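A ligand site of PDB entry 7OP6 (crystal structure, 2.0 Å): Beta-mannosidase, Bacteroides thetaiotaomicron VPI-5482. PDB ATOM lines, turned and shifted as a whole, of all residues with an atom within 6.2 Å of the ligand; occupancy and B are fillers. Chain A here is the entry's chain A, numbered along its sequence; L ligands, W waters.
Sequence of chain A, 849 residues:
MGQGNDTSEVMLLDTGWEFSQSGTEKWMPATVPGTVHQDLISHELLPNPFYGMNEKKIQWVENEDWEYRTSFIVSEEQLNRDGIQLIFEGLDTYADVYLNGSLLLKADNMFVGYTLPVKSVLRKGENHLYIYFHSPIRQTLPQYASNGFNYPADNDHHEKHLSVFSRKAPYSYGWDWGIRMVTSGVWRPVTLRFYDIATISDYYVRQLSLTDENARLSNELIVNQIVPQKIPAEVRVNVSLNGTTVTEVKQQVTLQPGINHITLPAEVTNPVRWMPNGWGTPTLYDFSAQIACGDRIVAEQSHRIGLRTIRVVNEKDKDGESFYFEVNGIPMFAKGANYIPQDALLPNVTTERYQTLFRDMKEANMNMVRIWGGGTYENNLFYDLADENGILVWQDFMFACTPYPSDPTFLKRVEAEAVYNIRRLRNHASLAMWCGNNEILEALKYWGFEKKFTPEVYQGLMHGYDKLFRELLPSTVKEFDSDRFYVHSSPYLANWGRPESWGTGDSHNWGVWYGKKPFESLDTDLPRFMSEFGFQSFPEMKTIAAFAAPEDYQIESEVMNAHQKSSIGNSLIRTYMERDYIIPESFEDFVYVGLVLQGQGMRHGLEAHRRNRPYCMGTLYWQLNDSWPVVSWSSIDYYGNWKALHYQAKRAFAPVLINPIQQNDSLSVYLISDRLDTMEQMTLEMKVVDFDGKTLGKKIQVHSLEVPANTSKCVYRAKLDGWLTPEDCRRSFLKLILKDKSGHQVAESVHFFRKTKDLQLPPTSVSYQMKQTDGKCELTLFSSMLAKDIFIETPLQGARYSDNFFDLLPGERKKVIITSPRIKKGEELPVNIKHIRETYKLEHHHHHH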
ATOM      1  N   ASN A 155       6.847 -21.943  30.388  1.00  0.00           N
ATOM      2  CA  ASN A 155       7.730 -22.217  29.224  1.00  0.00           C
ATOM      3  C   ASN A 155       9.200 -21.855  29.490  1.00  0.00           C
ATOM      4  O   ASN A 155      10.048 -22.260  28.669  1.00  0.00           O
ATOM      5  CB  ASN A 155       7.189 -21.534  27.971  1.00  0.00           C
ATOM      6  CG  ASN A 155       5.922 -22.226  27.506  1.00  0.00           C
ATOM      7  OD1 ASN A 155       5.997 -23.364  27.032  1.00  0.00           O
ATOM      8  ND2 ASN A 155       4.779 -21.588  27.664  1.00  0.00           N
ATOM      9  N   TRP A 175      10.544 -23.664  25.369  1.00  0.00           N
ATOM     10  CA  TRP A 175       9.111 -23.589  24.991  1.00  0.00           C
ATOM     11  C   TRP A 175       8.555 -25.012  24.904  1.00  0.00           C
ATOM     12  O   TRP A 175       9.372 -25.927  24.917  1.00  0.00           O
ATOM     13  CB  TRP A 175       8.855 -22.782  23.677  1.00  0.00           C
ATOM     14  CG  TRP A 175       7.510 -22.107  23.729  1.00  0.00           C
ATOM     15  CD1 TRP A 175       6.333 -22.572  23.222  1.00  0.00           C
ATOM     16  CD2 TRP A 175       7.189 -20.904  24.450  1.00  0.00           C
ATOM     17  NE1 TRP A 175       5.305 -21.732  23.545  1.00  0.00           N
ATOM     18  CE2 TRP A 175       5.795 -20.707  24.312  1.00  0.00           C
ATOM     19  CE3 TRP A 175       7.927 -19.964  25.168  1.00  0.00           C
ATOM     20  CZ2 TRP A 175       5.125 -19.615  24.880  1.00  0.00           C
ATOM     21  CZ3 TRP A 175       7.281 -18.883  25.713  1.00  0.00           C
ATOM     22  CH2 TRP A 175       5.900 -18.701  25.578  1.00  0.00           C
ATOM     23  N   ASP A 176       7.230 -25.204  24.788  1.00  0.00           N
ATOM     24  CA  ASP A 176       6.611 -26.546  24.824  1.00  0.00           C
ATOM     25  C   ASP A 176       6.836 -27.280  23.482  1.00  0.00           C
ATOM     26  O   ASP A 176       6.266 -28.389  23.315  1.00  0.00           O
ATOM     27  CB  ASP A 176       5.148 -26.488  25.307  1.00  0.00           C
ATOM     28  CG  ASP A 176       4.135 -25.755  24.425  1.00  0.00           C
ATOM     29  OD1 ASP A 176       4.517 -25.290  23.312  1.00  0.00           O
ATOM     30  OD2 ASP A 176       2.948 -25.673  24.860  1.00  0.00           O
ATOM     31  N   TRP A 177       7.654 -26.709  22.572  1.00  0.00           N
ATOM     32  CA  TRP A 177       8.228 -27.398  21.391  1.00  0.00           C
ATOM     33  C   TRP A 177       9.739 -27.156  21.288  1.00  0.00           C
ATOM     34  O   TRP A 177      10.268 -27.458  20.225  1.00  0.00           O
ATOM     35  CB  TRP A 177       7.554 -26.968  20.067  1.00  0.00           C
ATOM     36  CG  TRP A 177       7.325 -25.496  19.925  1.00  0.00           C
ATOM     37  CD1 TRP A 177       6.111 -24.881  19.975  1.00  0.00           C
ATOM     38  CD2 TRP A 177       8.299 -24.436  19.825  1.00  0.00           C
ATOM     39  NE1 TRP A 177       6.258 -23.523  19.868  1.00  0.00           N
ATOM     40  CE2 TRP A 177       7.577 -23.216  19.790  1.00  0.00           C
ATOM     41  CE3 TRP A 177       9.698 -24.376  19.738  1.00  0.00           C
ATOM     42  CZ2 TRP A 177       8.189 -21.967  19.685  1.00  0.00           C
ATOM     43  CZ3 TRP A 177      10.310 -23.146  19.608  1.00  0.00           C
ATOM     44  CH2 TRP A 177       9.561 -21.958  19.604  1.00  0.00           C
ATOM     45  N   ARG A 370       0.879 -15.655  10.867  1.00  0.00           N
ATOM     46  CA  ARG A 370       1.024 -14.952  12.153  1.00  0.00           C
ATOM     47  C   ARG A 370       2.457 -15.132  12.676  1.00  0.00           C
ATOM     48  O   ARG A 370       2.879 -16.279  12.900  1.00  0.00           O
ATOM     49  CB  ARG A 370      -0.026 -15.457  13.140  1.00  0.00           C
ATOM     50  CG  ARG A 370       0.160 -14.870  14.534  1.00  0.00           C
ATOM     51  CD  ARG A 370      -1.090 -15.043  15.363  1.00  0.00           C
ATOM     52  NE  ARG A 370      -0.818 -14.723  16.756  1.00  0.00           N
ATOM     53  CZ  ARG A 370      -1.088 -15.525  17.815  1.00  0.00           C
ATOM     54  NH1 ARG A 370      -1.616 -16.732  17.660  1.00  0.00           N
ATOM     55  NH2 ARG A 370      -0.758 -15.113  19.021  1.00  0.00           N
ATOM     56  N   TRP A 372       4.275 -15.192  15.693  1.00  0.00           N
ATOM     57  CA  TRP A 372       3.797 -15.432  17.074  1.00  0.00           C
ATOM     58  C   TRP A 372       4.768 -14.802  18.089  1.00  0.00           C
ATOM     59  O   TRP A 372       5.940 -14.791  17.805  1.00  0.00           O
ATOM     60  CB  TRP A 372       3.624 -16.955  17.226  1.00  0.00           C
ATOM     61  CG  TRP A 372       3.599 -17.449  18.630  1.00  0.00           C
ATOM     62  CD1 TRP A 372       2.518 -17.579  19.448  1.00  0.00           C
ATOM     63  CD2 TRP A 372       4.726 -17.948  19.351  1.00  0.00           C
ATOM     64  NE1 TRP A 372       2.905 -18.127  20.641  1.00  0.00           N
ATOM     65  CE2 TRP A 372       4.255 -18.347  20.621  1.00  0.00           C
ATOM     66  CE3 TRP A 372       6.090 -18.082  19.056  1.00  0.00           C
ATOM     67  CZ2 TRP A 372       5.107 -18.893  21.579  1.00  0.00           C
ATOM     68  CZ3 TRP A 372       6.928 -18.614  20.010  1.00  0.00           C
ATOM     69  CH2 TRP A 372       6.440 -19.006  21.259  1.00  0.00           C
ATOM     70  N   CYS A 401       2.275 -15.722  27.097  1.00  0.00           N
ATOM     71  CA  CYS A 401       1.856 -16.799  28.053  1.00  0.00           C
ATOM     72  C   CYS A 401       2.236 -16.526  29.521  1.00  0.00           C
ATOM     73  O   CYS A 401       1.887 -17.396  30.371  1.00  0.00           O
ATOM     74  CB  CYS A 401       2.446 -18.135  27.643  1.00  0.00           C
ATOM     75  SG  CYS A 401       1.795 -18.715  26.058  1.00  0.00           S
ATOM     76  N   ASN A 438       0.417 -12.933  23.075  1.00  0.00           N
ATOM     77  CA  ASN A 438      -0.196 -14.274  22.975  1.00  0.00           C
ATOM     78  C   ASN A 438      -0.698 -14.673  24.364  1.00  0.00           C
ATOM     79  O   ASN A 438       0.135 -14.881  25.243  1.00  0.00           O
ATOM     80  CB  ASN A 438       0.797 -15.278  22.387  1.00  0.00           C
ATOM     81  CG  ASN A 438       0.201 -16.655  22.244  1.00  0.00           C
ATOM     82  OD1 ASN A 438      -0.681 -16.885  21.402  1.00  0.00           O
ATOM     83  ND2 ASN A 438       0.650 -17.571  23.107  1.00  0.00           N
ATOM     84  N   GLU A 439      -2.016 -14.745  24.550  1.00  0.00           N
ATOM     85  CA  GLU A 439      -2.715 -15.461  25.665  1.00  0.00           C
ATOM     86  C   GLU A 439      -2.489 -14.850  27.062  1.00  0.00           C
ATOM     87  O   GLU A 439      -2.851 -15.519  28.049  1.00  0.00           O
ATOM     88  CB  GLU A 439      -2.285 -16.946  25.724  1.00  0.00           C
ATOM     89  CG  GLU A 439      -2.913 -17.779  24.612  1.00  0.00           C
ATOM     90  CD  GLU A 439      -2.277 -19.146  24.363  1.00  0.00           C
ATOM     91  OE1 GLU A 439      -1.279 -19.467  25.055  1.00  0.00           O
ATOM     92  OE2 GLU A 439      -2.772 -19.889  23.461  1.00  0.00           O
ATOM     93  N   TRP A 447      -6.093 -19.252  34.393  1.00  0.00           N
ATOM     94  CA  TRP A 447      -5.028 -20.272  34.621  1.00  0.00           C
ATOM     95  C   TRP A 447      -4.740 -20.425  36.119  1.00  0.00           C
ATOM     96  O   TRP A 447      -3.763 -21.102  36.449  1.00  0.00           O
ATOM     97  CB  TRP A 447      -3.765 -19.956  33.816  1.00  0.00           C
ATOM     98  CG  TRP A 447      -3.932 -20.103  32.335  1.00  0.00           C
ATOM     99  CD1 TRP A 447      -5.079 -20.393  31.632  1.00  0.00           C
ATOM    100  CD2 TRP A 447      -2.898 -19.933  31.343  1.00  0.00           C
ATOM    101  NE1 TRP A 447      -4.820 -20.431  30.288  1.00  0.00           N
ATOM    102  CE2 TRP A 447      -3.489 -20.144  30.082  1.00  0.00           C
ATOM    103  CE3 TRP A 447      -1.530 -19.615  31.416  1.00  0.00           C
ATOM    104  CZ2 TRP A 447      -2.757 -20.053  28.891  1.00  0.00           C
ATOM    105  CZ3 TRP A 447      -0.815 -19.507  30.243  1.00  0.00           C
ATOM    106  CH2 TRP A 447      -1.420 -19.729  28.991  1.00  0.00           C
ATOM    107  N   HIS A 508      -8.524 -19.487  20.295  1.00  0.00           N
ATOM    108  CA  HIS A 508      -7.482 -20.542  20.410  1.00  0.00           C
ATOM    109  C   HIS A 508      -8.165 -21.830  20.926  1.00  0.00           C
ATOM    110  O   HIS A 508      -8.394 -21.942  22.162  1.00  0.00           O
ATOM    111  CB  HIS A 508      -6.343 -20.093  21.345  1.00  0.00           C
ATOM    112  CG  HIS A 508      -5.491 -18.960  20.860  1.00  0.00           C
ATOM    113  ND1 HIS A 508      -4.217 -18.723  21.368  1.00  0.00           N
ATOM    114  CD2 HIS A 508      -5.726 -17.963  19.970  1.00  0.00           C
ATOM    115  CE1 HIS A 508      -3.716 -17.643  20.805  1.00  0.00           C
ATOM    116  NE2 HIS A 508      -4.603 -17.163  19.940  1.00  0.00           N
ATOM    117  N   TRP A 510      -7.982 -25.053  22.206  1.00  0.00           N
ATOM    118  CA  TRP A 510      -7.184 -26.097  22.915  1.00  0.00           C
ATOM    119  C   TRP A 510      -7.980 -27.398  23.117  1.00  0.00           C
ATOM    120  O   TRP A 510      -7.424 -28.297  23.748  1.00  0.00           O
ATOM    121  CB  TRP A 510      -6.742 -25.570  24.281  1.00  0.00           C
ATOM    122  CG  TRP A 510      -5.724 -24.474  24.333  1.00  0.00           C
ATOM    123  CD1 TRP A 510      -5.410 -23.553  23.368  1.00  0.00           C
ATOM    124  CD2 TRP A 510      -4.899 -24.159  25.462  1.00  0.00           C
ATOM    125  NE1 TRP A 510      -4.426 -22.724  23.824  1.00  0.00           N
ATOM    126  CE2 TRP A 510      -4.083 -23.073  25.095  1.00  0.00           C
ATOM    127  CE3 TRP A 510      -4.739 -24.732  26.739  1.00  0.00           C
ATOM    128  CZ2 TRP A 510      -3.139 -22.543  25.970  1.00  0.00           C
ATOM    129  CZ3 TRP A 510      -3.793 -24.217  27.598  1.00  0.00           C
ATOM    130  CH2 TRP A 510      -3.020 -23.117  27.223  1.00  0.00           C
ATOM    131  N   TRP A 513      -6.058 -31.838  21.232  1.00  0.00           N
ATOM    132  CA  TRP A 513      -4.787 -31.957  21.999  1.00  0.00           C
ATOM    133  C   TRP A 513      -5.055 -31.807  23.507  1.00  0.00           C
ATOM    134  O   TRP A 513      -5.411 -32.834  24.127  1.00  0.00           O
ATOM    135  CB  TRP A 513      -3.677 -31.025  21.468  1.00  0.00           C
ATOM    136  CG  TRP A 513      -2.328 -31.435  21.989  1.00  0.00           C
ATOM    137  CD1 TRP A 513      -1.598 -30.794  22.940  1.00  0.00           C
ATOM    138  CD2 TRP A 513      -1.597 -32.632  21.677  1.00  0.00           C
ATOM    139  NE1 TRP A 513      -0.440 -31.497  23.209  1.00  0.00           N
ATOM    140  CE2 TRP A 513      -0.421 -32.631  22.445  1.00  0.00           C
ATOM    141  CE3 TRP A 513      -1.816 -33.697  20.790  1.00  0.00           C
ATOM    142  CZ2 TRP A 513       0.537 -33.631  22.365  1.00  0.00           C
ATOM    143  CZ3 TRP A 513      -0.863 -34.699  20.723  1.00  0.00           C
ATOM    144  CH2 TRP A 513       0.283 -34.667  21.506  1.00  0.00           C
ATOM    145  N   TYR A 514      -4.878 -30.624  24.117  1.00  0.00           N
ATOM    146  CA  TYR A 514      -4.975 -30.433  25.592  1.00  0.00           C
ATOM    147  C   TYR A 514      -6.325 -30.948  26.136  1.00  0.00           C
ATOM    148  O   TYR A 514      -6.299 -31.556  27.201  1.00  0.00           O
ATOM    149  CB  TYR A 514      -4.666 -28.994  26.005  1.00  0.00           C
ATOM    150  CG  TYR A 514      -4.698 -28.675  27.476  1.00  0.00           C
ATOM    151  CD1 TYR A 514      -5.862 -28.302  28.112  1.00  0.00           C
ATOM    152  CD2 TYR A 514      -3.525 -28.669  28.220  1.00  0.00           C
ATOM    153  CE1 TYR A 514      -5.894 -27.983  29.461  1.00  0.00           C
ATOM    154  CE2 TYR A 514      -3.535 -28.368  29.583  1.00  0.00           C
ATOM    155  CZ  TYR A 514      -4.718 -28.006  30.194  1.00  0.00           C
ATOM    156  OH  TYR A 514      -4.749 -27.693  31.512  1.00  0.00           O
ATOM    157  N   GLU A 532      -5.542 -19.977  16.549  1.00  0.00           N
ATOM    158  CA  GLU A 532      -4.681 -21.135  16.938  1.00  0.00           C
ATOM    159  C   GLU A 532      -5.515 -22.420  17.119  1.00  0.00           C
ATOM    160  O   GLU A 532      -6.527 -22.384  17.847  1.00  0.00           O
ATOM    161  CB  GLU A 532      -3.907 -20.780  18.206  1.00  0.00           C
ATOM    162  CG  GLU A 532      -2.842 -21.802  18.602  1.00  0.00           C
ATOM    163  CD  GLU A 532      -2.501 -21.920  20.095  1.00  0.00           C
ATOM    164  OE1 GLU A 532      -3.366 -21.661  20.951  1.00  0.00           O
ATOM    165  OE2 GLU A 532      -1.164 -22.425  20.438  1.00  0.00           O
ATOM    166  N   GLY A 534      -4.444 -27.142  16.737  1.00  0.00           N
ATOM    167  CA  GLY A 534      -3.369 -28.030  16.258  1.00  0.00           C
ATOM    168  C   GLY A 534      -3.339 -29.421  16.876  1.00  0.00           C
ATOM    169  O   GLY A 534      -4.068 -29.673  17.848  1.00  0.00           O
ATOM    170  N   SER A 566       5.740 -31.001  25.629  1.00  0.00           N
ATOM    171  CA  SER A 566       4.338 -30.822  26.091  1.00  0.00           C
ATOM    172  C   SER A 566       4.071 -31.709  27.309  1.00  0.00           C
ATOM    173  O   SER A 566       4.643 -32.834  27.334  1.00  0.00           O
ATOM    174  CB  SER A 566       3.365 -31.118  24.974  1.00  0.00           C
ATOM    175  OG  SER A 566       2.121 -30.483  25.222  1.00  0.00           O
ATOM    176  N   TRP A 622      -1.762 -24.167  14.226  1.00  0.00           N
ATOM    177  CA  TRP A 622      -0.553 -24.288  15.052  1.00  0.00           C
ATOM    178  C   TRP A 622       0.065 -25.646  14.735  1.00  0.00           C
ATOM    179  O   TRP A 622      -0.579 -26.644  15.037  1.00  0.00           O
ATOM    180  CB  TRP A 622      -0.948 -24.144  16.501  1.00  0.00           C
ATOM    181  CG  TRP A 622       0.215 -24.131  17.434  1.00  0.00           C
ATOM    182  CD1 TRP A 622       0.743 -25.199  18.101  1.00  0.00           C
ATOM    183  CD2 TRP A 622       1.045 -22.993  17.754  1.00  0.00           C
ATOM    184  NE1 TRP A 622       1.825 -24.791  18.855  1.00  0.00           N
ATOM    185  CE2 TRP A 622       2.034 -23.454  18.655  1.00  0.00           C
ATOM    186  CE3 TRP A 622       1.011 -21.633  17.430  1.00  0.00           C
ATOM    187  CZ2 TRP A 622       2.982 -22.592  19.215  1.00  0.00           C
ATOM    188  CZ3 TRP A 622       1.962 -20.787  17.974  1.00  0.00           C
ATOM    189  CH2 TRP A 622       2.936 -21.269  18.843  1.00  0.00           C
ATOM    190  N   TRP A 633       3.715 -29.806  16.774  1.00  0.00           N
ATOM    191  CA  TRP A 633       2.478 -29.502  16.008  1.00  0.00           C
ATOM    192  C   TRP A 633       2.815 -29.075  14.565  1.00  0.00           C
ATOM    193  O   TRP A 633       1.872 -28.815  13.809  1.00  0.00           O
ATOM    194  CB  TRP A 633       1.647 -28.424  16.739  1.00  0.00           C
ATOM    195  CG  TRP A 633       1.224 -28.731  18.148  1.00  0.00           C
ATOM    196  CD1 TRP A 633       0.013 -29.240  18.526  1.00  0.00           C
ATOM    197  CD2 TRP A 633       1.928 -28.449  19.386  1.00  0.00           C
ATOM    198  NE1 TRP A 633      -0.077 -29.344  19.896  1.00  0.00           N
ATOM    199  CE2 TRP A 633       1.086 -28.880  20.451  1.00  0.00           C
ATOM    200  CE3 TRP A 633       3.175 -27.905  19.710  1.00  0.00           C
ATOM    201  CZ2 TRP A 633       1.458 -28.755  21.797  1.00  0.00           C
ATOM    202  CZ3 TRP A 633       3.562 -27.814  21.034  1.00  0.00           C
ATOM    203  CH2 TRP A 633       2.702 -28.229  22.062  1.00  0.00           C
HETATM  204  C1  LIG L   1      -0.704 -22.675  21.785  1.00  0.00           C
HETATM  205  C2  LIG L   1       0.292 -21.600  22.186  1.00  0.00           C
HETATM  206  C3  LIG L   1       0.889 -21.919  23.578  1.00  0.00           C
HETATM  207  C4  LIG L   1       1.573 -23.290  23.531  1.00  0.00           C
HETATM  208  C5  LIG L   1       0.679 -24.442  23.053  1.00  0.00           C
HETATM  209  C6  LIG L   1      -0.287 -24.984  24.138  1.00  0.00           C
HETATM  210  C7  LIG L   1      -0.046 -24.052  21.758  1.00  0.00           C
HETATM  211  O1  LIG L   1      -0.304 -20.276  22.100  1.00  0.00           O
HETATM  212  O2  LIG L   1      -0.096 -21.877  24.633  1.00  0.00           O
HETATM  213  O3  LIG L   1       2.684 -23.207  22.628  1.00  0.00           O
HETATM  214  O4  LIG L   1      -1.350 -25.794  23.546  1.00  0.00           O
HETATM  215  N1  LIG L   1      -1.101 -25.052  21.382  1.00  0.00           N
HETATM  216  O   HOH W   1      -3.015 -25.280  19.393  1.00  0.00           O
HETATM  217  O   HOH W   2      -1.229 -19.346  19.485  1.00  0.00           O
HETATM  218  O   HOH W   3       1.358 -22.149  27.132  1.00  0.00           O
HETATM  219  O   HOH W   4      -0.978 -27.898  25.418  1.00  0.00           O
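Merely in contact with the ligand: Trp 510, Trp 622 and Cys 401.
Hydrophobic or aromatic side chains within 4 Å of the ligand: Trp 175, Trp 510 and Trp 622.
Along chain A the residues within 4 Å of the ligand span positions 175 to 622.
The nearest printed residue that does not touch the ligand is Trp 372 (4.1 Å).
Water W3 lies within hydrogen-bond range of an oxygen (O2) of the ligand and the side-chain sulfur (SG) of Cys 401.
Water W2 lies within hydrogen-bond range of O1 of the ligand (2.9 Å), OD1 of Asn 438 (3.2 Å), NH1 of Arg 370 (3.2 Å) and OE2 of Glu 532 (3.2 Å).
NH2 of Arg 370 sits at hydrogen-bond distance from OD1 of Asn 438 (3.0 Å).
The indole nitrogen of Trp 510 is in hydrogen-bond range of the side-chain carboxylate of Glu 439 (3.3 Å).
N of Asp 176 is in hydrogen-bond range of OD1 of Asn 155 (3.2 Å).
SG of Cys 401 lies within hydrogen-bond range of OE1 of Glu 439 (3.3 Å).
The side-chain carboxylate of Glu 532 sits at hydrogen-bond distance from a ring nitrogen (ND1) of His 508, 3.1 Å away.
The side-chain amide nitrogen (ND2) of Asn 438 lies close to the indole nitrogen (NE1) of Trp 372 (3.4 Å).
The side-chain carboxylate of Glu 439 sits at hydrogen-bond distance from a ring nitrogen (ND1) of His 508 (2.8 Å).
The side-chain carboxylate (OE1) of Glu 439 lies within hydrogen-bond range of the side-chain amide nitrogen (ND2) of Asn 438 (3.3 Å).
An oxygen (O3) of the ligand sits at hydrogen-bond distance from the indole nitrogen of Trp 175, at 3.1 Å.
The side-chain carboxylate (OE1) of Glu 439 is in hydrogen-bond range of an oxygen (O2) of the ligand.
The side-chain amide nitrogen of Asn 438 lies within hydrogen-bond range of an oxygen (O1) of the ligand, 3.0 Å away.
An oxygen (O3) of the ligand sits at hydrogen-bond distance from the side-chain carboxylate (OD1) of Asp 176, at 2.9 Å.
The side-chain carboxylate (OE2) of Glu 532 is covalently linked to a carbon (C1) of the ligand (1.4 Å).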
